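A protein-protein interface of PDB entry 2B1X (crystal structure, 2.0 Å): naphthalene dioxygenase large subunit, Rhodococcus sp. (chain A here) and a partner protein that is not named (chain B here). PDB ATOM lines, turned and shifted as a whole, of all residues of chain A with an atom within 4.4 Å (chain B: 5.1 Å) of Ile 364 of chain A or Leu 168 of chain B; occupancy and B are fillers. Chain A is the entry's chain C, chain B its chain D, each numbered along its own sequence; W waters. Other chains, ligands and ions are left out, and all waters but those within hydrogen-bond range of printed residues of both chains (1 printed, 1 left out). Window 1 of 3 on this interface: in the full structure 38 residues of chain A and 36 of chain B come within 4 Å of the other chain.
Of the printed residues of chain B, Ile 364 of chain A touches His 66 (3.5 Å), Ile 163 (3.8 Å), Asn 167 (3.5 Å) and Leu 168 (2.8 Å).
Of the printed residues of chain A, His 66 of chain B touches Gln 195, Ile 364 and Ser 365.
Of the printed residues of chain B, Gln 195 of chain A touches His 66 (3.6 Å).
Gly 363 of chain A touches none of the printed residues of chain B.
Leu 134 of chain B touches none of the printed residues of chain A.
The nearest residue of chain B that does not touch Ile 364 of chain A is Thr 165 of chain B (4.8 Å).
The nearest printed residue of chain A that does not touch Leu 168 of chain B is Gly 366 of chain A (6.0 Å).
The nearest printed residue of chain A that does not touch His 166 of chain B is Ile 364 of chain A (5.2 Å).
OE1 of Gln 195 of chain A is in hydrogen-bond range of N of Ile 364 of chain A (2.8 Å).
O of Val 46 of chain B sits at hydrogen-bond distance from N of His 66 of chain B (2.8 Å).
The backbone NH (N) of Val 46 of chain B is in hydrogen-bond range of the backbone carbonyl oxygen (O) of Met 67 of chain B.
The backbone NH of Ala 169 of chain B lies close to the side-chain amide oxygen of Asn 167 of chain B (3.4 Å).
Water W1 lies within hydrogen-bond range of OG of Ser 365 of chain A and NH2 of Arg 77 of chain B.
His 66 of chain B touches Gln 195 of chain A.
CA of Trp 197 of chain A touches O of Ile 163 of chain B, 3.3 Å away.
O of Thr 165 of chain B touches CD1 of Trp 197 of chain A, at 3.4 Å.
His 66 of chain B touches Ile 364 of chain A.
CD1 of Ile 364 of chain A touches CB of Ile 163 of chain B, at 3.8 Å.
Asn 167 of chain B touches Ile 364 of chain A.
CE of Met 67 of chain B touches CB of Ser 365 of chain A, at 3.7 Å.
Ser 365 of chain A touches Leu 168 of chain B (CB to O, 3.8 Å).
The backbone carbonyl oxygen (O) of His 166 of chain B sits at hydrogen-bond distance from the indole nitrogen (NE1) of Trp 197 of chain A.
O of Ile 364 of chain A sits at hydrogen-bond distance from N of Leu 168 of chain B.
The backbone carbonyl oxygen (O) of His 66 of chain B is in hydrogen-bond range of the side-chain hydroxyl (OG) of Ser 365 of chain A (2.6 Å).
The backbone carbonyl oxygen (O) of Ser 365 of chain A lies within hydrogen-bond range of the guanidinium group (NH1) of Arg 77 of chain B (2.8 Å).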
ATOM      1  N   GLN A 195      19.417 -14.573 -23.554  1.00  0.00           N
ATOM      2  CA  GLN A 195      19.219 -13.455 -22.620  1.00  0.00           C
ATOM      3  C   GLN A 195      18.362 -12.428 -23.354  1.00  0.00           C
ATOM      4  O   GLN A 195      18.685 -12.036 -24.476  1.00  0.00           O
ATOM      5  CB  GLN A 195      20.526 -12.795 -22.266  1.00  0.00           C
ATOM      6  CG  GLN A 195      21.527 -13.627 -21.483  1.00  0.00           C
ATOM      7  CD  GLN A 195      22.825 -12.889 -21.323  1.00  0.00           C
ATOM      8  OE1 GLN A 195      22.978 -11.833 -21.893  1.00  0.00           O
ATOM      9  NE2 GLN A 195      23.760 -13.434 -20.553  1.00  0.00           N
ATOM     10  N   TRP A 197      16.645  -8.563 -22.819  1.00  0.00           N
ATOM     11  CA  TRP A 197      16.472  -7.359 -22.021  1.00  0.00           C
ATOM     12  C   TRP A 197      16.324  -6.133 -22.882  1.00  0.00           C
ATOM     13  O   TRP A 197      16.686  -6.141 -24.056  1.00  0.00           O
ATOM     14  CB  TRP A 197      17.703  -7.181 -21.084  1.00  0.00           C
ATOM     15  CG  TRP A 197      18.989  -6.687 -21.723  1.00  0.00           C
ATOM     16  CD1 TRP A 197      19.547  -5.410 -21.581  1.00  0.00           C
ATOM     17  CD2 TRP A 197      19.951  -7.441 -22.483  1.00  0.00           C
ATOM     18  NE1 TRP A 197      20.747  -5.339 -22.254  1.00  0.00           N
ATOM     19  CE2 TRP A 197      21.017  -6.562 -22.819  1.00  0.00           C
ATOM     20  CE3 TRP A 197      19.995  -8.761 -22.979  1.00  0.00           C
ATOM     21  CZ2 TRP A 197      22.130  -6.967 -23.596  1.00  0.00           C
ATOM     22  CZ3 TRP A 197      21.139  -9.173 -23.760  1.00  0.00           C
ATOM     23  CH2 TRP A 197      22.164  -8.269 -24.055  1.00  0.00           C
ATOM     24  N   PHE A 362      30.299 -10.523 -23.163  1.00  0.00           N
ATOM     25  CA  PHE A 362      29.108 -10.082 -23.893  1.00  0.00           C
ATOM     26  C   PHE A 362      27.809 -10.461 -23.193  1.00  0.00           C
ATOM     27  O   PHE A 362      27.832 -11.065 -22.129  1.00  0.00           O
ATOM     28  CB  PHE A 362      29.186 -10.509 -25.372  1.00  0.00           C
ATOM     29  CG  PHE A 362      30.174  -9.639 -26.166  1.00  0.00           C
ATOM     30  CD1 PHE A 362      31.566  -9.903 -26.114  1.00  0.00           C
ATOM     31  CD2 PHE A 362      29.724  -8.521 -26.886  1.00  0.00           C
ATOM     32  CE1 PHE A 362      32.469  -9.091 -26.765  1.00  0.00           C
ATOM     33  CE2 PHE A 362      30.648  -7.687 -27.579  1.00  0.00           C
ATOM     34  CZ  PHE A 362      32.019  -7.963 -27.495  1.00  0.00           C
ATOM     35  N   GLY A 363      26.674 -10.044 -23.722  1.00  0.00           N
ATOM     36  CA  GLY A 363      25.437 -10.307 -23.003  1.00  0.00           C
ATOM     37  C   GLY A 363      25.204  -9.203 -21.983  1.00  0.00           C
ATOM     38  O   GLY A 363      26.005  -8.251 -21.876  1.00  0.00           O
ATOM     39  N   ILE A 364      24.127  -9.352 -21.225  1.00  0.00           N
ATOM     40  CA  ILE A 364      23.594  -8.308 -20.344  1.00  0.00           C
ATOM     41  C   ILE A 364      24.544  -7.829 -19.221  1.00  0.00           C
ATOM     42  O   ILE A 364      24.530  -6.631 -18.814  1.00  0.00           O
ATOM     43  CB  ILE A 364      22.229  -8.818 -19.757  1.00  0.00           C
ATOM     44  CG1 ILE A 364      21.371  -7.649 -19.282  1.00  0.00           C
ATOM     45  CG2 ILE A 364      22.450  -9.833 -18.623  1.00  0.00           C
ATOM     46  CD1 ILE A 364      20.068  -8.082 -18.552  1.00  0.00           C
ATOM     47  N   SER A 365      25.337  -8.750 -18.699  1.00  0.00           N
ATOM     48  CA  SER A 365      26.311  -8.391 -17.666  1.00  0.00           C
ATOM     49  C   SER A 365      27.765  -8.416 -18.136  1.00  0.00           C
ATOM     50  O   SER A 365      28.689  -8.283 -17.323  1.00  0.00           O
ATOM     51  CB  SER A 365      26.129  -9.288 -16.418  1.00  0.00           C
ATOM     52  OG  SER A 365      26.444 -10.630 -16.745  1.00  0.00           O
ATOM     53  N   GLY A 366      27.984  -8.576 -19.437  1.00  0.00           N
ATOM     54  CA  GLY A 366      29.348  -8.665 -19.962  1.00  0.00           C
ATOM     55  C   GLY A 366      30.092  -7.343 -19.830  1.00  0.00           C
ATOM     56  O   GLY A 366      29.475  -6.276 -19.961  1.00  0.00           O
ATOM     57  N   VAL B  46      22.797 -15.122 -11.531  1.00  0.00           N
ATOM     58  CA  VAL B  46      21.518 -14.547 -11.889  1.00  0.00           C
ATOM     59  C   VAL B  46      20.949 -15.398 -13.059  1.00  0.00           C
ATOM     60  O   VAL B  46      21.340 -15.230 -14.210  1.00  0.00           O
ATOM     61  CB  VAL B  46      21.734 -13.075 -12.334  1.00  0.00           C
ATOM     62  CG1 VAL B  46      20.407 -12.389 -12.660  1.00  0.00           C
ATOM     63  CG2 VAL B  46      22.518 -12.290 -11.240  1.00  0.00           C
ATOM     64  N   HIS B  66      22.170 -15.034 -16.869  1.00  0.00           N
ATOM     65  CA  HIS B  66      22.495 -13.605 -17.068  1.00  0.00           C
ATOM     66  C   HIS B  66      23.878 -13.249 -16.506  1.00  0.00           C
ATOM     67  O   HIS B  66      24.549 -12.324 -16.991  1.00  0.00           O
ATOM     68  CB  HIS B  66      21.450 -12.676 -16.424  1.00  0.00           C
ATOM     69  CG  HIS B  66      20.134 -12.703 -17.120  1.00  0.00           C
ATOM     70  ND1 HIS B  66      19.991 -12.364 -18.450  1.00  0.00           N
ATOM     71  CD2 HIS B  66      18.907 -13.067 -16.689  1.00  0.00           C
ATOM     72  CE1 HIS B  66      18.729 -12.536 -18.814  1.00  0.00           C
ATOM     73  NE2 HIS B  66      18.053 -12.958 -17.760  1.00  0.00           N
ATOM     74  N   MET B  67      24.286 -13.981 -15.483  1.00  0.00           N
ATOM     75  CA  MET B  67      25.516 -13.714 -14.750  1.00  0.00           C
ATOM     76  C   MET B  67      25.848 -14.984 -13.974  1.00  0.00           C
ATOM     77  O   MET B  67      24.942 -15.609 -13.386  1.00  0.00           O
ATOM     78  CB  MET B  67      25.313 -12.529 -13.798  1.00  0.00           C
ATOM     79  CG  MET B  67      26.614 -12.010 -13.169  1.00  0.00           C
ATOM     80  SD  MET B  67      26.306 -10.521 -12.065  1.00  0.00           S
ATOM     81  CE  MET B  67      25.230  -9.668 -12.895  1.00  0.00           C
ATOM     82  N   ARG B  77      35.355  -7.688 -12.504  1.00  0.00           N
ATOM     83  CA  ARG B  77      34.211  -6.760 -12.499  1.00  0.00           C
ATOM     84  C   ARG B  77      34.527  -5.483 -11.702  1.00  0.00           C
ATOM     85  O   ARG B  77      34.319  -4.338 -12.177  1.00  0.00           O
ATOM     86  CB  ARG B  77      32.953  -7.505 -11.965  1.00  0.00           C
ATOM     87  CG  ARG B  77      31.602  -6.882 -12.319  1.00  0.00           C
ATOM     88  CD  ARG B  77      30.365  -7.750 -11.987  1.00  0.00           C
ATOM     89  NE  ARG B  77      30.393  -9.062 -12.676  1.00  0.00           N
ATOM     90  CZ  ARG B  77      30.044  -9.263 -13.957  1.00  0.00           C
ATOM     91  NH1 ARG B  77      29.641  -8.246 -14.730  1.00  0.00           N
ATOM     92  NH2 ARG B  77      30.086 -10.490 -14.473  1.00  0.00           N
ATOM     93  N   LEU B 134      14.385  -3.332 -10.473  1.00  0.00           N
ATOM     94  CA  LEU B 134      14.499  -4.788 -10.521  1.00  0.00           C
ATOM     95  C   LEU B 134      13.924  -5.340  -9.219  1.00  0.00           C
ATOM     96  O   LEU B 134      14.175  -4.801  -8.143  1.00  0.00           O
ATOM     97  CB  LEU B 134      15.947  -5.249 -10.704  1.00  0.00           C
ATOM     98  CG  LEU B 134      16.695  -4.776 -11.961  1.00  0.00           C
ATOM     99  CD1 LEU B 134      18.085  -5.369 -11.993  1.00  0.00           C
ATOM    100  CD2 LEU B 134      15.925  -5.249 -13.211  1.00  0.00           C
ATOM    101  N   LEU B 158      15.260 -13.009 -10.386  1.00  0.00           N
ATOM    102  CA  LEU B 158      14.430 -11.831 -10.645  1.00  0.00           C
ATOM    103  C   LEU B 158      13.011 -12.208 -11.021  1.00  0.00           C
ATOM    104  O   LEU B 158      12.820 -13.237 -11.623  1.00  0.00           O
ATOM    105  CB  LEU B 158      15.055 -11.000 -11.774  1.00  0.00           C
ATOM    106  CG  LEU B 158      16.492 -10.533 -11.461  1.00  0.00           C
ATOM    107  CD1 LEU B 158      17.136  -9.861 -12.685  1.00  0.00           C
ATOM    108  CD2 LEU B 158      16.472  -9.547 -10.245  1.00  0.00           C
ATOM    109  N   ILE B 163      14.443  -8.730 -19.019  1.00  0.00           N
ATOM    110  CA  ILE B 163      14.924  -7.856 -17.939  1.00  0.00           C
ATOM    111  C   ILE B 163      14.684  -6.395 -18.272  1.00  0.00           C
ATOM    112  O   ILE B 163      14.926  -5.961 -19.414  1.00  0.00           O
ATOM    113  CB  ILE B 163      16.423  -8.096 -17.665  1.00  0.00           C
ATOM    114  CG1 ILE B 163      16.680  -9.572 -17.396  1.00  0.00           C
ATOM    115  CG2 ILE B 163      16.955  -7.157 -16.501  1.00  0.00           C
ATOM    116  CD1 ILE B 163      15.827 -10.207 -16.339  1.00  0.00           C
ATOM    117  N   THR B 165      16.073  -3.441 -17.377  1.00  0.00           N
ATOM    118  CA  THR B 165      17.102  -2.419 -17.333  1.00  0.00           C
ATOM    119  C   THR B 165      18.073  -2.700 -18.481  1.00  0.00           C
ATOM    120  O   THR B 165      18.036  -3.789 -19.059  1.00  0.00           O
ATOM    121  CB  THR B 165      17.719  -2.298 -15.910  1.00  0.00           C
ATOM    122  OG1 THR B 165      18.566  -1.152 -15.835  1.00  0.00           O
ATOM    123  CG2 THR B 165      18.626  -3.510 -15.524  1.00  0.00           C
ATOM    124  N   HIS B 166      18.838  -1.686 -18.880  1.00  0.00           N
ATOM    125  CA  HIS B 166      19.669  -1.722 -20.096  1.00  0.00           C
ATOM    126  C   HIS B 166      20.997  -2.491 -19.975  1.00  0.00           C
ATOM    127  O   HIS B 166      21.636  -2.789 -20.985  1.00  0.00           O
ATOM    128  CB  HIS B 166      19.915  -0.291 -20.617  1.00  0.00           C
ATOM    129  CG  HIS B 166      20.680   0.562 -19.645  1.00  0.00           C
ATOM    130  ND1 HIS B 166      20.062   1.228 -18.614  1.00  0.00           N
ATOM    131  CD2 HIS B 166      22.015   0.794 -19.501  1.00  0.00           C
ATOM    132  CE1 HIS B 166      20.976   1.841 -17.875  1.00  0.00           C
ATOM    133  NE2 HIS B 166      22.165   1.608 -18.397  1.00  0.00           N
ATOM    134  N   ASN B 167      21.425  -2.794 -18.749  1.00  0.00           N
ATOM    135  CA  ASN B 167      22.558  -3.724 -18.508  1.00  0.00           C
ATOM    136  C   ASN B 167      22.535  -4.162 -17.043  1.00  0.00           C
ATOM    137  O   ASN B 167      21.799  -3.592 -16.233  1.00  0.00           O
ATOM    138  CB  ASN B 167      23.948  -3.127 -18.892  1.00  0.00           C
ATOM    139  CG  ASN B 167      24.218  -1.756 -18.220  1.00  0.00           C
ATOM    140  OD1 ASN B 167      23.782  -1.516 -17.105  1.00  0.00           O
ATOM    141  ND2 ASN B 167      24.902  -0.865 -18.924  1.00  0.00           N
ATOM    142  N   LEU B 168      23.318  -5.170 -16.700  1.00  0.00           N
ATOM    143  CA  LEU B 168      23.460  -5.532 -15.313  1.00  0.00           C
ATOM    144  C   LEU B 168      24.856  -5.126 -14.904  1.00  0.00           C
ATOM    145  O   LEU B 168      25.684  -5.966 -14.591  1.00  0.00           O
ATOM    146  CB  LEU B 168      23.194  -7.017 -15.084  1.00  0.00           C
ATOM    147  CG  LEU B 168      21.757  -7.533 -15.257  1.00  0.00           C
ATOM    148  CD1 LEU B 168      21.720  -9.001 -14.975  1.00  0.00           C
ATOM    149  CD2 LEU B 168      20.800  -6.832 -14.339  1.00  0.00           C
ATOM    150  N   ALA B 169      25.083  -3.817 -14.924  1.00  0.00           N
ATOM    151  CA  ALA B 169      26.330  -3.198 -14.492  1.00  0.00           C
ATOM    152  C   ALA B 169      26.414  -3.071 -12.972  1.00  0.00           C
ATOM    153  O   ALA B 169      27.496  -2.849 -12.435  1.00  0.00           O
ATOM    154  CB  ALA B 169      26.485  -1.816 -15.146  1.00  0.00           C
ATOM    155  N   LEU B 170      25.288  -3.218 -12.283  1.00  0.00           N
ATOM    156  CA  LEU B 170      25.256  -3.115 -10.811  1.00  0.00           C
ATOM    157  C   LEU B 170      25.220  -4.483 -10.144  1.00  0.00           C
ATOM    158  O   LEU B 170      24.510  -5.390 -10.601  1.00  0.00           O
ATOM    159  CB  LEU B 170      24.028  -2.296 -10.341  1.00  0.00           C
ATOM    160  CG  LEU B 170      23.881  -0.849 -10.811  1.00  0.00           C
ATOM    161  CD1 LEU B 170      22.499  -0.297 -10.359  1.00  0.00           C
ATOM    162  CD2 LEU B 170      24.997  -0.007 -10.251  1.00  0.00           C
ATOM    163  N   MET B 172      23.926  -6.941  -7.405  1.00  0.00           N
ATOM    164  CA  MET B 172      22.680  -7.053  -6.657  1.00  0.00           C
ATOM    165  C   MET B 172      22.835  -7.804  -5.346  1.00  0.00           C
ATOM    166  O   MET B 172      23.585  -8.798  -5.277  1.00  0.00           O
ATOM    167  CB  MET B 172      21.621  -7.777  -7.512  1.00  0.00           C
ATOM    168  CG  MET B 172      21.086  -6.941  -8.657  1.00  0.00           C
ATOM    169  SD  MET B 172      20.479  -7.882 -10.072  1.00  0.00           S
ATOM    170  CE  MET B 172      21.991  -8.498 -10.743  1.00  0.00           C
ATOM    171  OXT MET B 172      22.162  -7.447  -4.373  1.00  0.00           O
HETATM  172  O   HOH W   1      28.938 -11.841 -16.761  1.00  0.00           O
